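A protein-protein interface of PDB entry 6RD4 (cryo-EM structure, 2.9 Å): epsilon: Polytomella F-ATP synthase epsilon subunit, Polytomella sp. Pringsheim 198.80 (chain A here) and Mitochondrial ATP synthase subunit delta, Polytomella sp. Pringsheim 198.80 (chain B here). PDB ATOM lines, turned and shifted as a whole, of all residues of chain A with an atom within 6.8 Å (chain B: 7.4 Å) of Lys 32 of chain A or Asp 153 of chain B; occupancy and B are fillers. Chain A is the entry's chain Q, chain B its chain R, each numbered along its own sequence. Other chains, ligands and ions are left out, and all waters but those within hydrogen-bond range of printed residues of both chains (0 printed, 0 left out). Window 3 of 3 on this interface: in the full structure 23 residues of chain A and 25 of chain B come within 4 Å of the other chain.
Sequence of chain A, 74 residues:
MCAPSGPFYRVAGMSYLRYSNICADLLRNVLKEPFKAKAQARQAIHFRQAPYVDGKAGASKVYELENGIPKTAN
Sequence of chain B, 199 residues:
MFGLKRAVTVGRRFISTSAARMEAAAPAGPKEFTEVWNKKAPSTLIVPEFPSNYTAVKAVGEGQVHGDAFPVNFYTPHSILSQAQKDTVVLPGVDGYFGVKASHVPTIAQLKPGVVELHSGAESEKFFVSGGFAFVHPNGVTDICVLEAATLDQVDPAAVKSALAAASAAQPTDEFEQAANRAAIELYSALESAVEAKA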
ATOM      1  N   ARG A  28       1.992  21.726  12.274  1.00  0.00           N
ATOM      2  CA  ARG A  28       1.658  23.130  12.499  1.00  0.00           C
ATOM      3  C   ARG A  28       0.753  23.689  11.411  1.00  0.00           C
ATOM      4  O   ARG A  28      -0.039  24.597  11.679  1.00  0.00           O
ATOM      5  CB  ARG A  28       2.930  23.969  12.600  1.00  0.00           C
ATOM      6  CG  ARG A  28       3.823  23.604  13.768  1.00  0.00           C
ATOM      7  CD  ARG A  28       5.000  24.543  13.871  1.00  0.00           C
ATOM      8  NE  ARG A  28       6.049  23.985  14.711  1.00  0.00           N
ATOM      9  CZ  ARG A  28       7.177  23.485  14.239  1.00  0.00           C
ATOM     10  NH1 ARG A  28       7.404  23.487  12.934  1.00  0.00           N
ATOM     11  NH2 ARG A  28       8.080  22.985  15.069  1.00  0.00           N
ATOM     12  N   VAL A  30      -1.793  22.362  10.260  1.00  0.00           N
ATOM     13  CA  VAL A  30      -3.104  21.777  10.490  1.00  0.00           C
ATOM     14  C   VAL A  30      -3.726  22.340  11.777  1.00  0.00           C
ATOM     15  O   VAL A  30      -4.877  22.038  12.114  1.00  0.00           O
ATOM     16  CB  VAL A  30      -2.957  20.233  10.482  1.00  0.00           C
ATOM     17  CG1 VAL A  30      -4.238  19.435  10.602  1.00  0.00           C
ATOM     18  CG2 VAL A  30      -2.271  19.798   9.207  1.00  0.00           C
ATOM     19  N   LEU A  31      -3.036  23.257  12.446  1.00  0.00           N
ATOM     20  CA  LEU A  31      -3.556  23.777  13.699  1.00  0.00           C
ATOM     21  C   LEU A  31      -4.663  24.811  13.480  1.00  0.00           C
ATOM     22  O   LEU A  31      -4.864  25.344  12.382  1.00  0.00           O
ATOM     23  CB  LEU A  31      -2.443  24.390  14.543  1.00  0.00           C
ATOM     24  CG  LEU A  31      -2.042  23.575  15.769  1.00  0.00           C
ATOM     25  CD1 LEU A  31      -1.458  22.270  15.330  1.00  0.00           C
ATOM     26  CD2 LEU A  31      -1.063  24.327  16.657  1.00  0.00           C
ATOM     27  N   LYS A  32      -5.389  25.067  14.570  1.00  0.00           N
ATOM     28  CA  LYS A  32      -6.368  26.143  14.654  1.00  0.00           C
ATOM     29  C   LYS A  32      -5.677  27.488  14.468  1.00  0.00           C
ATOM     30  O   LYS A  32      -4.548  27.676  14.917  1.00  0.00           O
ATOM     31  CB  LYS A  32      -7.043  26.088  16.023  1.00  0.00           C
ATOM     32  CG  LYS A  32      -8.146  27.073  16.272  1.00  0.00           C
ATOM     33  CD  LYS A  32      -8.494  27.112  17.752  1.00  0.00           C
ATOM     34  CE  LYS A  32      -9.263  25.886  18.180  1.00  0.00           C
ATOM     35  NZ  LYS A  32      -9.600  25.905  19.629  1.00  0.00           N
ATOM     36  N   GLU A  33      -6.363  28.434  13.811  1.00  0.00           N
ATOM     37  CA  GLU A  33      -5.762  29.717  13.438  1.00  0.00           C
ATOM     38  C   GLU A  33      -5.423  30.657  14.604  1.00  0.00           C
ATOM     39  O   GLU A  33      -4.425  31.382  14.499  1.00  0.00           O
ATOM     40  CB  GLU A  33      -6.655  30.430  12.413  1.00  0.00           C
ATOM     41  CG  GLU A  33      -6.000  31.615  11.698  1.00  0.00           C
ATOM     42  CD  GLU A  33      -4.664  31.287  11.032  1.00  0.00           C
ATOM     43  OE1 GLU A  33      -3.816  32.200  10.950  1.00  0.00           O
ATOM     44  OE2 GLU A  33      -4.479  30.157  10.528  1.00  0.00           O
ATOM     45  N   PRO A  34      -6.153  30.678  15.730  1.00  0.00           N
ATOM     46  CA  PRO A  34      -5.579  31.302  16.941  1.00  0.00           C
ATOM     47  C   PRO A  34      -4.293  30.659  17.449  1.00  0.00           C
ATOM     48  O   PRO A  34      -3.604  31.270  18.277  1.00  0.00           O
ATOM     49  CB  PRO A  34      -6.705  31.165  17.966  1.00  0.00           C
ATOM     50  CG  PRO A  34      -7.906  31.308  17.155  1.00  0.00           C
ATOM     51  CD  PRO A  34      -7.625  30.620  15.852  1.00  0.00           C
ATOM     52  N   PHE A  35      -3.951  29.454  16.995  1.00  0.00           N
ATOM     53  CA  PHE A  35      -2.718  28.802  17.380  1.00  0.00           C
ATOM     54  C   PHE A  35      -1.803  28.473  16.211  1.00  0.00           C
ATOM     55  O   PHE A  35      -0.668  28.053  16.445  1.00  0.00           O
ATOM     56  CB  PHE A  35      -3.039  27.524  18.160  1.00  0.00           C
ATOM     57  CG  PHE A  35      -3.883  27.770  19.367  1.00  0.00           C
ATOM     58  CD1 PHE A  35      -3.299  28.177  20.558  1.00  0.00           C
ATOM     59  CD2 PHE A  35      -5.255  27.623  19.313  1.00  0.00           C
ATOM     60  CE1 PHE A  35      -4.075  28.412  21.678  1.00  0.00           C
ATOM     61  CE2 PHE A  35      -6.037  27.855  20.417  1.00  0.00           C
ATOM     62  CZ  PHE A  35      -5.446  28.250  21.607  1.00  0.00           C
ATOM     63  N   LYS A  36      -2.257  28.649  14.969  1.00  0.00           N
ATOM     64  CA  LYS A  36      -1.432  28.307  13.814  1.00  0.00           C
ATOM     65  C   LYS A  36      -0.363  29.360  13.557  1.00  0.00           C
ATOM     66  O   LYS A  36       0.771  29.028  13.193  1.00  0.00           O
ATOM     67  CB  LYS A  36      -2.311  28.131  12.576  1.00  0.00           C
ATOM     68  CG  LYS A  36      -1.561  27.681  11.332  1.00  0.00           C
ATOM     69  CD  LYS A  36      -2.497  27.502  10.152  1.00  0.00           C
ATOM     70  CE  LYS A  36      -1.752  27.019   8.922  1.00  0.00           C
ATOM     71  NZ  LYS A  36      -0.798  28.043   8.434  1.00  0.00           N
ATOM     72  N   ALA A  37      -0.703  30.637  13.735  1.00  0.00           N
ATOM     73  CA  ALA A  37       0.251  31.702  13.448  1.00  0.00           C
ATOM     74  C   ALA A  37       1.277  31.859  14.557  1.00  0.00           C
ATOM     75  O   ALA A  37       2.406  32.281  14.292  1.00  0.00           O
ATOM     76  CB  ALA A  37      -0.478  33.025  13.217  1.00  0.00           C
ATOM     77  N   LYS A  38       0.908  31.560  15.803  1.00  0.00           N
ATOM     78  CA  LYS A  38       1.893  31.604  16.878  1.00  0.00           C
ATOM     79  C   LYS A  38       2.824  30.403  16.805  1.00  0.00           C
ATOM     80  O   LYS A  38       3.954  30.445  17.303  1.00  0.00           O
ATOM     81  CB  LYS A  38       1.195  31.685  18.236  1.00  0.00           C
ATOM     82  CG  LYS A  38       0.380  30.461  18.600  1.00  0.00           C
ATOM     83  CD  LYS A  38      -0.307  30.622  19.940  1.00  0.00           C
ATOM     84  CE  LYS A  38       0.707  30.653  21.068  1.00  0.00           C
ATOM     85  NZ  LYS A  38       1.428  29.367  21.194  1.00  0.00           N
ATOM     86  N   LYS B 126      -5.536  14.780  26.022  1.00  0.00           N
ATOM     87  CA  LYS B 126      -5.089  14.068  24.829  1.00  0.00           C
ATOM     88  C   LYS B 126      -4.308  15.014  23.928  1.00  0.00           C
ATOM     89  O   LYS B 126      -4.895  15.851  23.238  1.00  0.00           O
ATOM     90  CB  LYS B 126      -6.274  13.467  24.085  1.00  0.00           C
ATOM     91  CG  LYS B 126      -7.036  12.418  24.871  1.00  0.00           C
ATOM     92  CD  LYS B 126      -8.153  11.815  24.034  1.00  0.00           C
ATOM     93  CE  LYS B 126      -9.040  10.905  24.864  1.00  0.00           C
ATOM     94  NZ  LYS B 126      -8.353   9.664  25.303  1.00  0.00           N
ATOM     95  N   ALA B 150       0.595  19.178  19.789  1.00  0.00           N
ATOM     96  CA  ALA B 150      -0.652  19.916  19.754  1.00  0.00           C
ATOM     97  C   ALA B 150      -1.748  19.122  20.443  1.00  0.00           C
ATOM     98  O   ALA B 150      -1.879  17.918  20.219  1.00  0.00           O
ATOM     99  CB  ALA B 150      -1.058  20.206  18.315  1.00  0.00           C
ATOM    100  N   THR B 151      -2.517  19.787  21.288  1.00  0.00           N
ATOM    101  CA  THR B 151      -3.766  19.196  21.731  1.00  0.00           C
ATOM    102  C   THR B 151      -4.737  19.187  20.557  1.00  0.00           C
ATOM    103  O   THR B 151      -4.688  20.049  19.679  1.00  0.00           O
ATOM    104  CB  THR B 151      -4.339  19.973  22.918  1.00  0.00           C
ATOM    105  OG1 THR B 151      -3.273  20.326  23.801  1.00  0.00           O
ATOM    106  CG2 THR B 151      -5.315  19.130  23.709  1.00  0.00           C
ATOM    107  N   LEU B 152      -5.612  18.186  20.529  1.00  0.00           N
ATOM    108  CA  LEU B 152      -6.569  18.036  19.440  1.00  0.00           C
ATOM    109  C   LEU B 152      -7.661  19.093  19.451  1.00  0.00           C
ATOM    110  O   LEU B 152      -8.399  19.204  18.466  1.00  0.00           O
ATOM    111  CB  LEU B 152      -7.184  16.645  19.513  1.00  0.00           C
ATOM    112  CG  LEU B 152      -6.230  15.574  18.997  1.00  0.00           C
ATOM    113  CD1 LEU B 152      -6.682  14.227  19.461  1.00  0.00           C
ATOM    114  CD2 LEU B 152      -6.177  15.625  17.477  1.00  0.00           C
ATOM    115  N   ASP B 153      -7.775  19.870  20.532  1.00  0.00           N
ATOM    116  CA  ASP B 153      -8.743  20.954  20.583  1.00  0.00           C
ATOM    117  C   ASP B 153      -8.375  22.067  19.620  1.00  0.00           C
ATOM    118  O   ASP B 153      -9.261  22.751  19.099  1.00  0.00           O
ATOM    119  CB  ASP B 153      -8.824  21.502  22.003  1.00  0.00           C
ATOM    120  CG  ASP B 153      -9.228  20.445  23.003  1.00  0.00           C
ATOM    121  OD1 ASP B 153      -9.899  19.477  22.594  1.00  0.00           O
ATOM    122  OD2 ASP B 153      -8.870  20.579  24.192  1.00  0.00           O
ATOM    123  N   GLN B 154      -7.081  22.242  19.345  1.00  0.00           N
ATOM    124  CA  GLN B 154      -6.593  23.288  18.459  1.00  0.00           C
ATOM    125  C   GLN B 154      -6.136  22.747  17.112  1.00  0.00           C
ATOM    126  O   GLN B 154      -5.286  23.358  16.461  1.00  0.00           O
ATOM    127  CB  GLN B 154      -5.473  24.074  19.140  1.00  0.00           C
ATOM    128  CG  GLN B 154      -4.248  23.287  19.528  1.00  0.00           C
ATOM    129  CD  GLN B 154      -3.299  24.091  20.385  1.00  0.00           C
ATOM    130  OE1 GLN B 154      -3.704  25.038  21.054  1.00  0.00           O
ATOM    131  NE2 GLN B 154      -2.027  23.720  20.367  1.00  0.00           N
ATOM    132  N   VAL B 155      -6.669  21.623  16.688  1.00  0.00           N
ATOM    133  CA  VAL B 155      -6.447  21.102  15.345  1.00  0.00           C
ATOM    134  C   VAL B 155      -7.761  21.201  14.583  1.00  0.00           C
ATOM    135  O   VAL B 155      -8.833  20.961  15.150  1.00  0.00           O
ATOM    136  CB  VAL B 155      -5.921  19.651  15.411  1.00  0.00           C
ATOM    137  CG1 VAL B 155      -5.586  19.121  14.031  1.00  0.00           C
ATOM    138  CG2 VAL B 155      -4.714  19.565  16.328  1.00  0.00           C
ATOM    139  N   ASP B 156      -7.697  21.592  13.297  1.00  0.00           N
ATOM    140  CA  ASP B 156      -9.010  21.483  12.667  1.00  0.00           C
ATOM    141  C   ASP B 156      -9.075  20.289  11.718  1.00  0.00           C
ATOM    142  O   ASP B 156      -8.110  20.006  10.999  1.00  0.00           O
ATOM    143  CB  ASP B 156      -9.401  22.765  11.920  1.00  0.00           C
ATOM    144  CG  ASP B 156      -8.256  23.391  11.135  1.00  0.00           C
ATOM    145  OD1 ASP B 156      -7.333  22.686  10.690  1.00  0.00           O
ATOM    146  OD2 ASP B 156      -8.302  24.622  10.949  1.00  0.00           O
ATOM    147  N   LYS B 198     -13.586  11.062  19.330  1.00  0.00           N
ATOM    148  CA  LYS B 198     -13.497  11.929  20.494  1.00  0.00           C
ATOM    149  C   LYS B 198     -14.799  11.883  21.284  1.00  0.00           C
ATOM    150  O   LYS B 198     -15.881  11.728  20.709  1.00  0.00           O
ATOM    151  CB  LYS B 198     -13.174  13.363  20.066  1.00  0.00           C
ATOM    152  CG  LYS B 198     -11.917  13.527  19.189  1.00  0.00           C
ATOM    153  CD  LYS B 198     -10.595  13.245  19.918  1.00  0.00           C
ATOM    154  CE  LYS B 198      -9.992  11.885  19.554  1.00  0.00           C
ATOM    155  NZ  LYS B 198      -8.700  11.643  20.244  1.00  0.00           N
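Of the printed residues of chain B, Val 30 of chain A touches Val 155 and Asp 156.
Of chain B, only Asp 153 (3.2 Å) and Gln 154 (2.6 Å) come within 4 Å of Lys 32 of chain A.
Asp 153 of chain B touches one residue of chain A.
Of the printed residues of chain A, Val 155 of chain B touches Val 30 (3.6 Å).
The nearest residue of chain A that does not touch Asp 153 of chain B is Phe 35 of chain A (6.2 Å).
The nearest printed residue of chain A that does not touch Gln 154 of chain B is Val 30 of chain A (4.6 Å).
Of the 10 printed residues of chain A, 4 touch a printed residue of chain B.
Printed residues of chain A that touch a printed residue of chain B: Val 30, Leu 31, Lys 32 and Phe 35.
Hydrophobic or aromatic side chains of chain A that line the printed part of chain B: Val 30, Leu 31 and Phe 35.
Among the printed residues, 8 pairs touch across the chains.
Among the printed residues, no Asp or Glu carboxylate lies within 4 Å of a Lys or Arg side-chain nitrogen of the other chain.
The backbone carbonyl oxygen (O) of Val 30 of chain A lies within hydrogen-bond range of the backbone NH (N) of Asp 156 of chain B (3.1 Å).
The side-chain amino group (NZ) of Lys 32 of chain A is in hydrogen-bond range of the backbone carbonyl oxygen (O) of Asp 153 of chain B.
The backbone carbonyl oxygen (O) of Gln 154 of chain B is in hydrogen-bond range of the backbone NH (N) of Lys 32 of chain A (2.6 Å).
Among the printed residues, pairs that only touch across the chains: Val 30 of chain A with Val 155 of chain B, Leu 31 of chain A with Ala 150 of chain B, Leu 31 of chain A with Gln 154 of chain B, Leu 31 of chain A with Asp 156 of chain B and Phe 35 of chain A with Gln 154 of chain B.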
